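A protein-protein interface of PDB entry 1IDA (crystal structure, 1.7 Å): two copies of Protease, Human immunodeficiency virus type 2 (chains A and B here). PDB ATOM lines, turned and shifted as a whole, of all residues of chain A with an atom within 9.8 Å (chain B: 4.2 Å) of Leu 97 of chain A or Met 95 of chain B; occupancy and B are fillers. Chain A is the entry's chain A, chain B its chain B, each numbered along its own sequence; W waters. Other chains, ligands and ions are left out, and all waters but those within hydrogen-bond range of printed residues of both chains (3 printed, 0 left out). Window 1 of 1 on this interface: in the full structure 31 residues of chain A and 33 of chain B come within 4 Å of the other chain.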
ATOM      1  N   PRO A   1      -4.718  20.232 -17.061  1.00  0.00           N
ATOM      2  CA  PRO A   1      -4.879  19.855 -15.666  1.00  0.00           C
ATOM      3  C   PRO A   1      -3.562  19.613 -14.915  1.00  0.00           C
ATOM      4  O   PRO A   1      -2.558  19.300 -15.539  1.00  0.00           O
ATOM      5  CB  PRO A   1      -5.697  18.566 -15.664  1.00  0.00           C
ATOM      6  CG  PRO A   1      -6.329  18.470 -17.032  1.00  0.00           C
ATOM      7  CD  PRO A   1      -5.638  19.477 -17.941  1.00  0.00           C
ATOM      8  N   GLN A   2      -3.608  19.728 -13.546  1.00  0.00           N
ATOM      9  CA  GLN A   2      -2.489  19.466 -12.672  1.00  0.00           C
ATOM     10  C   GLN A   2      -2.916  18.565 -11.556  1.00  0.00           C
ATOM     11  O   GLN A   2      -4.004  18.711 -11.023  1.00  0.00           O
ATOM     12  CB  GLN A   2      -1.769  20.649 -12.028  1.00  0.00           C
ATOM     13  CG  GLN A   2      -1.847  21.981 -12.732  1.00  0.00           C
ATOM     14  CD  GLN A   2      -0.886  22.931 -12.006  1.00  0.00           C
ATOM     15  OE1 GLN A   2      -1.128  24.155 -11.862  1.00  0.00           O
ATOM     16  NE2 GLN A   2       0.128  22.326 -11.370  1.00  0.00           N
ATOM     17  N   PHE A   3      -2.049  17.663 -11.165  1.00  0.00           N
ATOM     18  CA  PHE A   3      -2.375  16.760 -10.100  1.00  0.00           C
ATOM     19  C   PHE A   3      -1.328  16.881  -9.032  1.00  0.00           C
ATOM     20  O   PHE A   3      -0.136  16.658  -9.322  1.00  0.00           O
ATOM     21  CB  PHE A   3      -2.418  15.269 -10.512  1.00  0.00           C
ATOM     22  CG  PHE A   3      -3.449  14.959 -11.563  1.00  0.00           C
ATOM     23  CD1 PHE A   3      -3.209  15.236 -12.913  1.00  0.00           C
ATOM     24  CD2 PHE A   3      -4.620  14.266 -11.246  1.00  0.00           C
ATOM     25  CE1 PHE A   3      -4.121  14.924 -13.925  1.00  0.00           C
ATOM     26  CE2 PHE A   3      -5.544  13.921 -12.240  1.00  0.00           C
ATOM     27  CZ  PHE A   3      -5.307  14.282 -13.570  1.00  0.00           C
ATOM     28  N   SER A   4      -1.771  17.270  -7.820  1.00  0.00           N
ATOM     29  CA  SER A   4      -0.864  17.320  -6.717  1.00  0.00           C
ATOM     30  C   SER A   4      -0.727  15.851  -6.280  1.00  0.00           C
ATOM     31  O   SER A   4      -1.579  14.980  -6.573  1.00  0.00           O
ATOM     32  CB  SER A   4      -1.306  18.263  -5.621  1.00  0.00           C
ATOM     33  OG  SER A   4      -2.073  17.519  -4.709  1.00  0.00           O
ATOM     34  N   LEU A   5       0.346  15.467  -5.699  1.00  0.00           N
ATOM     35  CA  LEU A   5       0.364  14.013  -5.504  1.00  0.00           C
ATOM     36  C   LEU A   5      -0.039  13.531  -4.104  1.00  0.00           C
ATOM     37  O   LEU A   5       0.272  12.406  -3.706  1.00  0.00           O
ATOM     38  CB  LEU A   5       1.730  13.439  -5.928  1.00  0.00           C
ATOM     39  CG  LEU A   5       1.994  13.727  -7.411  1.00  0.00           C
ATOM     40  CD1 LEU A   5       3.464  13.664  -7.741  1.00  0.00           C
ATOM     41  CD2 LEU A   5       1.111  12.791  -8.265  1.00  0.00           C
ATOM     42  N   TRP A   6      -0.778  14.378  -3.383  1.00  0.00           N
ATOM     43  CA  TRP A   6      -1.318  14.051  -2.058  1.00  0.00           C
ATOM     44  C   TRP A   6      -2.205  12.811  -2.131  1.00  0.00           C
ATOM     45  O   TRP A   6      -2.093  11.966  -1.297  1.00  0.00           O
ATOM     46  CB  TRP A   6      -1.989  15.321  -1.418  1.00  0.00           C
ATOM     47  CG  TRP A   6      -2.551  15.052  -0.060  1.00  0.00           C
ATOM     48  CD1 TRP A   6      -3.882  14.980   0.278  1.00  0.00           C
ATOM     49  CD2 TRP A   6      -1.810  14.834   1.162  1.00  0.00           C
ATOM     50  NE1 TRP A   6      -4.014  14.611   1.607  1.00  0.00           N
ATOM     51  CE2 TRP A   6      -2.765  14.600   2.194  1.00  0.00           C
ATOM     52  CE3 TRP A   6      -0.446  14.871   1.488  1.00  0.00           C
ATOM     53  CZ2 TRP A   6      -2.377  14.351   3.524  1.00  0.00           C
ATOM     54  CZ3 TRP A   6      -0.076  14.655   2.798  1.00  0.00           C
ATOM     55  CH2 TRP A   6      -1.037  14.379   3.781  1.00  0.00           C
ATOM     56  N   LYS A   7      -3.131  12.703  -3.111  1.00  0.00           N
ATOM     57  CA  LYS A   7      -3.941  11.508  -3.359  1.00  0.00           C
ATOM     58  C   LYS A   7      -3.420  10.809  -4.618  1.00  0.00           C
ATOM     59  O   LYS A   7      -2.771  11.455  -5.389  1.00  0.00           O
ATOM     60  CB  LYS A   7      -5.363  11.882  -3.707  1.00  0.00           C
ATOM     61  CG  LYS A   7      -6.014  12.793  -2.674  1.00  0.00           C
ATOM     62  CD  LYS A   7      -6.174  12.119  -1.319  1.00  0.00           C
ATOM     63  CE  LYS A   7      -7.010  12.945  -0.317  1.00  0.00           C
ATOM     64  NZ  LYS A   7      -8.424  13.241  -0.719  1.00  0.00           N
ATOM     65  N   PRO A   9      -3.191   9.886  -8.280  1.00  0.00           N
ATOM     66  CA  PRO A   9      -3.677  10.568  -9.484  1.00  0.00           C
ATOM     67  C   PRO A   9      -4.541   9.603 -10.362  1.00  0.00           C
ATOM     68  O   PRO A   9      -4.036   8.945 -11.262  1.00  0.00           O
ATOM     69  CB  PRO A   9      -2.381  10.978 -10.168  1.00  0.00           C
ATOM     70  CG  PRO A   9      -1.344   9.957  -9.727  1.00  0.00           C
ATOM     71  CD  PRO A   9      -1.781   9.502  -8.350  1.00  0.00           C
ATOM     72  N   LEU A  24      -2.504   7.244 -13.174  1.00  0.00           N
ATOM     73  CA  LEU A  24      -1.504   7.822 -14.034  1.00  0.00           C
ATOM     74  C   LEU A  24      -0.144   7.580 -13.402  1.00  0.00           C
ATOM     75  O   LEU A  24       0.230   8.199 -12.390  1.00  0.00           O
ATOM     76  CB  LEU A  24      -1.826   9.333 -14.266  1.00  0.00           C
ATOM     77  CG  LEU A  24      -3.293   9.623 -14.601  1.00  0.00           C
ATOM     78  CD1 LEU A  24      -3.542  11.151 -14.671  1.00  0.00           C
ATOM     79  CD2 LEU A  24      -3.617   8.956 -15.931  1.00  0.00           C
ATOM     80  N   ASP A  25       0.580   6.665 -14.017  1.00  0.00           N
ATOM     81  CA  ASP A  25       1.789   6.064 -13.471  1.00  0.00           C
ATOM     82  C   ASP A  25       3.060   6.345 -14.223  1.00  0.00           C
ATOM     83  O   ASP A  25       3.351   5.607 -15.163  1.00  0.00           O
ATOM     84  CB  ASP A  25       1.551   4.541 -13.273  1.00  0.00           C
ATOM     85  CG  ASP A  25       2.494   3.877 -12.247  1.00  0.00           C
ATOM     86  OD1 ASP A  25       3.504   4.638 -11.957  1.00  0.00           O
ATOM     87  OD2 ASP A  25       2.562   2.695 -12.018  1.00  0.00           O
ATOM     88  N   THR A  26       3.863   7.340 -13.726  1.00  0.00           N
ATOM     89  CA  THR A  26       5.184   7.691 -14.353  1.00  0.00           C
ATOM     90  C   THR A  26       6.213   6.579 -14.138  1.00  0.00           C
ATOM     91  O   THR A  26       7.243   6.526 -14.816  1.00  0.00           O
ATOM     92  CB  THR A  26       5.795   9.019 -13.757  1.00  0.00           C
ATOM     93  OG1 THR A  26       5.922   8.886 -12.361  1.00  0.00           O
ATOM     94  CG2 THR A  26       4.927  10.203 -14.000  1.00  0.00           C
ATOM     95  N   GLY A  27       5.950   5.659 -13.172  1.00  0.00           N
ATOM     96  CA  GLY A  27       6.929   4.623 -12.894  1.00  0.00           C
ATOM     97  C   GLY A  27       6.757   3.370 -13.734  1.00  0.00           C
ATOM     98  O   GLY A  27       7.593   2.476 -13.689  1.00  0.00           O
ATOM     99  N   ARG A  87       3.917   5.083 -18.975  1.00  0.00           N
ATOM    100  CA  ARG A  87       4.551   6.087 -19.825  1.00  0.00           C
ATOM    101  C   ARG A  87       4.184   6.050 -21.312  1.00  0.00           C
ATOM    102  O   ARG A  87       4.190   7.078 -21.975  1.00  0.00           O
ATOM    103  CB  ARG A  87       6.058   6.115 -19.691  1.00  0.00           C
ATOM    104  CG  ARG A  87       6.464   6.485 -18.252  1.00  0.00           C
ATOM    105  CD  ARG A  87       7.959   6.554 -18.138  1.00  0.00           C
ATOM    106  NE  ARG A  87       8.619   5.262 -18.457  1.00  0.00           N
ATOM    107  CZ  ARG A  87       9.265   4.982 -19.592  1.00  0.00           C
ATOM    108  NH1 ARG A  87       9.340   5.845 -20.602  1.00  0.00           N
ATOM    109  NH2 ARG A  87       9.848   3.794 -19.736  1.00  0.00           N
ATOM    110  N   LEU A  90       0.965   8.132 -21.144  1.00  0.00           N
ATOM    111  CA  LEU A  90       1.263   9.440 -20.599  1.00  0.00           C
ATOM    112  C   LEU A  90       2.003  10.269 -21.655  1.00  0.00           C
ATOM    113  O   LEU A  90       1.746  11.460 -21.819  1.00  0.00           O
ATOM    114  CB  LEU A  90       2.145   9.305 -19.338  1.00  0.00           C
ATOM    115  CG  LEU A  90       1.384   9.212 -18.024  1.00  0.00           C
ATOM    116  CD1 LEU A  90      -0.060   8.765 -18.122  1.00  0.00           C
ATOM    117  CD2 LEU A  90       2.218   8.630 -16.908  1.00  0.00           C
ATOM    118  N   THR A  91       2.962   9.619 -22.355  1.00  0.00           N
ATOM    119  CA  THR A  91       3.718  10.284 -23.424  1.00  0.00           C
ATOM    120  C   THR A  91       2.849  10.767 -24.598  1.00  0.00           C
ATOM    121  O   THR A  91       2.868  11.900 -24.995  1.00  0.00           O
ATOM    122  CB  THR A  91       4.863   9.396 -23.949  1.00  0.00           C
ATOM    123  OG1 THR A  91       5.777   9.264 -22.915  1.00  0.00           O
ATOM    124  CG2 THR A  91       5.548  10.101 -25.103  1.00  0.00           C
ATOM    125  N   GLY A  94       0.835  13.687 -23.732  1.00  0.00           N
ATOM    126  CA  GLY A  94       1.640  14.870 -23.537  1.00  0.00           C
ATOM    127  C   GLY A  94       1.720  15.324 -22.081  1.00  0.00           C
ATOM    128  O   GLY A  94       1.923  16.527 -21.856  1.00  0.00           O
ATOM    129  N   MET A  95       1.646  14.416 -21.120  1.00  0.00           N
ATOM    130  CA  MET A  95       1.812  14.781 -19.711  1.00  0.00           C
ATOM    131  C   MET A  95       3.259  14.907 -19.338  1.00  0.00           C
ATOM    132  O   MET A  95       4.137  14.308 -19.960  1.00  0.00           O
ATOM    133  CB  MET A  95       1.260  13.683 -18.823  1.00  0.00           C
ATOM    134  CG  MET A  95      -0.217  13.539 -19.070  1.00  0.00           C
ATOM    135  SD  MET A  95      -1.071  12.754 -17.648  1.00  0.00           S
ATOM    136  CE  MET A  95      -1.249  14.127 -16.492  1.00  0.00           C
ATOM    137  N   SER A  96       3.507  15.651 -18.321  1.00  0.00           N
ATOM    138  CA  SER A  96       4.856  15.831 -17.775  1.00  0.00           C
ATOM    139  C   SER A  96       4.825  15.859 -16.223  1.00  0.00           C
ATOM    140  O   SER A  96       3.800  16.167 -15.632  1.00  0.00           O
ATOM    141  CB  SER A  96       5.541  17.101 -18.275  1.00  0.00           C
ATOM    142  OG  SER A  96       4.781  18.238 -17.873  1.00  0.00           O
ATOM    143  N   LEU A  97       5.982  15.555 -15.644  1.00  0.00           N
ATOM    144  CA  LEU A  97       6.263  15.595 -14.248  1.00  0.00           C
ATOM    145  C   LEU A  97       7.041  16.888 -14.089  1.00  0.00           C
ATOM    146  O   LEU A  97       8.021  17.140 -14.817  1.00  0.00           O
ATOM    147  CB  LEU A  97       7.202  14.456 -13.893  1.00  0.00           C
ATOM    148  CG  LEU A  97       6.683  13.385 -12.967  1.00  0.00           C
ATOM    149  CD1 LEU A  97       7.917  12.641 -12.437  1.00  0.00           C
ATOM    150  CD2 LEU A  97       5.902  13.952 -11.787  1.00  0.00           C
ATOM    151  N   ASN A  98       6.559  17.758 -13.191  1.00  0.00           N
ATOM    152  CA  ASN A  98       7.134  19.043 -13.024  1.00  0.00           C
ATOM    153  C   ASN A  98       7.402  19.372 -11.569  1.00  0.00           C
ATOM    154  O   ASN A  98       6.630  18.999 -10.693  1.00  0.00           O
ATOM    155  CB  ASN A  98       6.117  20.059 -13.559  1.00  0.00           C
ATOM    156  CG  ASN A  98       5.790  19.853 -15.046  1.00  0.00           C
ATOM    157  OD1 ASN A  98       4.935  19.007 -15.412  1.00  0.00           O
ATOM    158  ND2 ASN A  98       6.495  20.605 -15.896  1.00  0.00           N
ATOM    159  N   LEU A  99       8.441  20.153 -11.353  1.00  0.00           N
ATOM    160  CA  LEU A  99       8.795  20.622 -10.051  1.00  0.00           C
ATOM    161  C   LEU A  99       9.208  22.082 -10.130  1.00  0.00           C
ATOM    162  O   LEU A  99       8.677  22.962  -9.401  1.00  0.00           O
ATOM    163  CB  LEU A  99       9.916  19.759  -9.518  1.00  0.00           C
ATOM    164  CG  LEU A  99      10.576  20.373  -8.314  1.00  0.00           C
ATOM    165  CD1 LEU A  99       9.556  20.255  -7.213  1.00  0.00           C
ATOM    166  CD2 LEU A  99      11.790  19.532  -7.940  1.00  0.00           C
ATOM    167  OXT LEU A  99      10.027  22.473 -11.010  1.00  0.00           O
ATOM    168  N   PRO B   1      12.246  22.178 -12.837  1.00  0.00           N
ATOM    169  CA  PRO B   1      12.505  21.018 -13.691  1.00  0.00           C
ATOM    170  C   PRO B   1      11.246  20.375 -14.213  1.00  0.00           C
ATOM    171  O   PRO B   1      10.240  20.385 -13.521  1.00  0.00           O
ATOM    172  CB  PRO B   1      13.310  20.005 -12.879  1.00  0.00           C
ATOM    173  CG  PRO B   1      13.960  20.819 -11.790  1.00  0.00           C
ATOM    174  CD  PRO B   1      13.199  22.155 -11.711  1.00  0.00           C
ATOM    175  N   GLN B   2      11.296  19.903 -15.479  1.00  0.00           N
ATOM    176  CA  GLN B   2      10.178  19.245 -16.118  1.00  0.00           C
ATOM    177  C   GLN B   2      10.697  17.964 -16.718  1.00  0.00           C
ATOM    178  O   GLN B   2      11.866  17.939 -17.138  1.00  0.00           O
ATOM    179  CB  GLN B   2       9.554  20.112 -17.192  1.00  0.00           C
ATOM    180  CG  GLN B   2       8.288  19.425 -17.664  1.00  0.00           C
ATOM    181  CD  GLN B   2       7.577  20.176 -18.771  1.00  0.00           C
ATOM    182  OE1 GLN B   2       7.303  21.386 -18.616  1.00  0.00           O
ATOM    183  NE2 GLN B   2       7.311  19.472 -19.913  1.00  0.00           N
ATOM    184  N   PHE B   3       9.904  16.897 -16.688  1.00  0.00           N
ATOM    185  CA  PHE B   3      10.333  15.625 -17.228  1.00  0.00           C
ATOM    186  C   PHE B   3       9.314  15.115 -18.227  1.00  0.00           C
ATOM    187  O   PHE B   3       8.148  14.915 -17.869  1.00  0.00           O
ATOM    188  CB  PHE B   3      10.450  14.544 -16.137  1.00  0.00           C
ATOM    189  CG  PHE B   3      11.528  14.831 -15.121  1.00  0.00           C
ATOM    190  CD1 PHE B   3      11.360  15.841 -14.165  1.00  0.00           C
ATOM    191  CD2 PHE B   3      12.685  14.049 -15.081  1.00  0.00           C
ATOM    192  CE1 PHE B   3      12.358  16.139 -13.237  1.00  0.00           C
ATOM    193  CE2 PHE B   3      13.684  14.313 -14.137  1.00  0.00           C
ATOM    194  CZ  PHE B   3      13.532  15.387 -13.254  1.00  0.00           C
ATOM    195  N   LEU B  24      11.151   8.454 -10.243  1.00  0.00           N
ATOM    196  CA  LEU B  24      10.077   9.329  -9.723  1.00  0.00           C
ATOM    197  C   LEU B  24       8.771   8.687 -10.138  1.00  0.00           C
ATOM    198  O   LEU B  24       8.390   8.698 -11.311  1.00  0.00           O
ATOM    199  CB  LEU B  24      10.190  10.767 -10.246  1.00  0.00           C
ATOM    200  CG  LEU B  24      11.622  11.332 -10.021  1.00  0.00           C
ATOM    201  CD1 LEU B  24      11.831  12.730 -10.684  1.00  0.00           C
ATOM    202  CD2 LEU B  24      11.931  11.332  -8.539  1.00  0.00           C
ATOM    203  N   THR B  26       4.769   8.232  -9.665  1.00  0.00           N
ATOM    204  CA  THR B  26       3.429   8.665  -9.239  1.00  0.00           C
ATOM    205  C   THR B  26       2.490   7.526  -8.890  1.00  0.00           C
ATOM    206  O   THR B  26       1.469   7.720  -8.248  1.00  0.00           O
ATOM    207  CB  THR B  26       2.733   9.595 -10.261  1.00  0.00           C
ATOM    208  OG1 THR B  26       2.595   8.930 -11.489  1.00  0.00           O
ATOM    209  CG2 THR B  26       3.479  10.921 -10.475  1.00  0.00           C
ATOM    210  N   LEU B  67      16.932  16.698  -6.538  1.00  0.00           N
ATOM    211  CA  LEU B  67      16.460  17.836  -7.311  1.00  0.00           C
ATOM    212  C   LEU B  67      16.739  19.165  -6.608  1.00  0.00           C
ATOM    213  O   LEU B  67      15.942  20.101  -6.609  1.00  0.00           O
ATOM    214  CB  LEU B  67      14.954  17.606  -7.610  1.00  0.00           C
ATOM    215  CG  LEU B  67      14.716  16.351  -8.488  1.00  0.00           C
ATOM    216  CD1 LEU B  67      13.240  16.063  -8.576  1.00  0.00           C
ATOM    217  CD2 LEU B  67      15.239  16.618  -9.902  1.00  0.00           C
ATOM    218  N   LEU B  90       7.455  12.725  -3.455  1.00  0.00           N
ATOM    219  CA  LEU B  90       7.111  13.675  -4.477  1.00  0.00           C
ATOM    220  C   LEU B  90       6.330  14.870  -3.923  1.00  0.00           C
ATOM    221  O   LEU B  90       6.462  16.001  -4.374  1.00  0.00           O
ATOM    222  CB  LEU B  90       6.383  13.030  -5.679  1.00  0.00           C
ATOM    223  CG  LEU B  90       7.155  11.847  -6.308  1.00  0.00           C
ATOM    224  CD1 LEU B  90       6.428  11.287  -7.527  1.00  0.00           C
ATOM    225  CD2 LEU B  90       8.544  12.247  -6.699  1.00  0.00           C
ATOM    226  N   LEU B  93       8.420  17.313  -2.103  1.00  0.00           N
ATOM    227  CA  LEU B  93       9.220  18.121  -2.992  1.00  0.00           C
ATOM    228  C   LEU B  93       8.404  19.193  -3.737  1.00  0.00           C
ATOM    229  O   LEU B  93       8.966  20.071  -4.371  1.00  0.00           O
ATOM    230  CB  LEU B  93       9.972  17.292  -4.066  1.00  0.00           C
ATOM    231  CG  LEU B  93      10.870  16.191  -3.579  1.00  0.00           C
ATOM    232  CD1 LEU B  93      11.294  15.342  -4.766  1.00  0.00           C
ATOM    233  CD2 LEU B  93      12.124  16.772  -2.965  1.00  0.00           C
ATOM    234  N   GLY B  94       7.058  19.046  -3.732  1.00  0.00           N
ATOM    235  CA  GLY B  94       6.181  19.917  -4.411  1.00  0.00           C
ATOM    236  C   GLY B  94       6.094  19.538  -5.890  1.00  0.00           C
ATOM    237  O   GLY B  94       5.894  20.387  -6.730  1.00  0.00           O
ATOM    238  N   MET B  95       6.275  18.270  -6.234  1.00  0.00           N
ATOM    239  CA  MET B  95       6.202  17.877  -7.620  1.00  0.00           C
ATOM    240  C   MET B  95       4.745  17.681  -8.059  1.00  0.00           C
ATOM    241  O   MET B  95       3.899  17.364  -7.221  1.00  0.00           O
ATOM    242  CB  MET B  95       7.073  16.598  -7.653  1.00  0.00           C
ATOM    243  CG  MET B  95       7.478  16.096  -9.020  1.00  0.00           C
ATOM    244  SD  MET B  95       9.063  15.265  -8.885  1.00  0.00           S
ATOM    245  CE  MET B  95       9.679  15.734 -10.494  1.00  0.00           C
ATOM    246  N   SER B  96       4.385  17.919  -9.338  1.00  0.00           N
ATOM    247  CA  SER B  96       3.015  17.666  -9.790  1.00  0.00           C
ATOM    248  C   SER B  96       3.039  17.000 -11.181  1.00  0.00           C
ATOM    249  O   SER B  96       4.050  17.066 -11.893  1.00  0.00           O
ATOM    250  CB  SER B  96       2.182  18.932  -9.869  1.00  0.00           C
ATOM    251  OG  SER B  96       2.846  19.814 -10.751  1.00  0.00           O
HETATM  252  O   HOH W   1       2.390  17.507  -5.091  1.00  0.00           O
HETATM  253  O   HOH W   2       7.205  23.083  -6.673  1.00  0.00           O
HETATM  254  O   HOH W   3       4.801  21.515  -9.437  1.00  0.00           O
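The backbone carbonyl oxygen (O) of Leu 24 of chain A is in hydrogen-bond range of the side-chain hydroxyl (OG1) of Thr 26 of chain B (2.6 Å).
The backbone carbonyl oxygen of Leu 24 of chain B sits at hydrogen-bond distance from the side-chain hydroxyl of Thr 26 of chain A (2.7 Å).
The side-chain hydroxyl (OG1) of Thr 26 of chain A is in hydrogen-bond range of the backbone NH (N) of Thr 26 of chain B, 3.0 Å away.
OG of Ser 96 of chain A sits close to NE2 of Gln 2 of chain B (3.5 Å).
N of Phe 3 of chain B lies within hydrogen-bond range of O of Leu 97 of chain A, 2.7 Å away.
The side-chain amide nitrogen (ND2) of Asn 98 of chain A sits close to the side-chain amide oxygen (OE1) of Gln 2 of chain B (2.9 Å).
The backbone carbonyl oxygen of Asn 98 of chain A is in hydrogen-bond range of the backbone NH of Ser 96 of chain B, 2.8 Å away.
The backbone carbonyl oxygen (O) of Pro 1 of chain B lies within hydrogen-bond range of the backbone NH (N) of Leu 99 of chain A (2.8 Å).
Leu 97 of chain A touches just these residues of chain B: Gln 2, Phe 3, Leu 24, Met 95 and Ser 96.
Of chain A, only Leu 5, Leu 97, Asn 98 and Leu 99 come within 4 Å of Met 95 of chain B.
Leu 24 of chain B touches just these residues of chain A: Thr 26 and Leu 97.
Leu 90 of chain B touches one residue of chain A.
Of chain A, only Leu 99 comes within 4 Å of Gly 94 of chain B.
Printed residues of chain B within 4 Å of Phe 3 of chain A: Ser 96 (3.3 Å).
Printed residues of chain B within 4 Å of Thr 26 of chain A: Leu 24 and Thr 26.
Gly 27 of chain A touches none of the printed residues of chain B.
The nearest printed residue of chain B that does not touch Leu 99 of chain A is Gln 2 of chain B (5.0 Å).
Water W1 lies within hydrogen-bond range of O of Met 95 of chain B (2.6 Å) and N of Leu 5 of chain A (3.0 Å).
Water W3 lies within hydrogen-bond range of OG of Ser 96 of chain B (2.9 Å), O of Gly 94 of chain B (3.1 Å) and O of Asn 98 of chain A (3.4 Å).
Water W2 bridges O of Gly 94 of chain B and O of Leu 99 of chain A.
Of the 11 printed residues of chain B, 11 touch a printed residue of chain A.
Printed residues of chain B that touch a printed residue of chain A: Pro 1, Gln 2, Phe 3, Leu 24, Thr 26, Leu 67, Leu 90, Leu 93, Gly 94, Met 95 and Ser 96.
Hydrophobic or aromatic side chains of chain B that line the printed part of chain A: Pro 1, Phe 3, Leu 24, Leu 67, Leu 90 and Met 95.
Of the 21 printed residues of chain A, 11 touch a printed residue of chain B.
Hydrophobic or aromatic side chains of chain A that line the printed part of chain B: Leu 5, Pro 9, Leu 97 and Leu 99.
Along chain A the printed residues that touch a printed residue of chain B span positions 2 to 99.
Among the printed residues, merely in contact across the chains: Gln 2 of chain A with Ser 96 of chain B, Phe 3 of chain A with Ser 96 of chain B, Leu 5 of chain A with Thr 26 of chain B, Leu 5 of chain A with Leu 90 of chain B, Leu 5 of chain A with Met 95 of chain B, Pro 9 of chain A with Thr 26 of chain B, Asp 25 of chain A with Thr 26 of chain B, Ser 96 of chain A with Phe 3 of chain B, Ser 96 of chain A with Ser 96 of chain B, Leu 97 of chain A with Gln 2 of chain B, Leu 97 of chain A with Leu 24 of chain B, Leu 97 of chain A with Met 95 of chain B, Leu 97 of chain A with Ser 96 of chain B, Asn 98 of chain A with Pro 1 of chain B, Asn 98 of chain A with Met 95 of chain B, Leu 99 of chain A with Leu 67 of chain B, Leu 99 of chain A with Leu 93 of chain B, Leu 99 of chain A with Gly 94 of chain B and Leu 99 of chain A with Met 95 of chain B.
The backbone carbonyl oxygen of Pro 9 of chain A lies within hydrogen-bond range of the backbone NH of Leu 24 of chain A (3.0 Å).
The side-chain carboxylate of Asp 25 of chain A is in hydrogen-bond range of the backbone NH of Gly 27 of chain A, at 2.9 Å.
The side-chain amide oxygen (OD1) of Asn 98 of chain A lies within hydrogen-bond range of the side-chain hydroxyl (OG) of Ser 96 of chain A, at 2.6 Å.
N of Met 95 of chain B lies within hydrogen-bond range of O of Leu 90 of chain B (2.9 Å).
Gln 2 of chain A touches Ser 96 of chain B, and with the chains exchanged Ser 96 of chain A touches Gln 2 of chain B.
Phe 3 of chain A touches Ser 96 of chain B, and with the chains exchanged Ser 96 of chain A touches Phe 3 of chain B.
Leu 24 of chain A touches Thr 26 of chain B, and with the chains exchanged Thr 26 of chain A touches Leu 24 of chain B.
Thr 26 of chain A touches its own counterpart, Thr 26 of chain B.
Of the 27 pairs that touch across the chains among the printed residues, 8 have their exchanged pair printed and touching as well.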
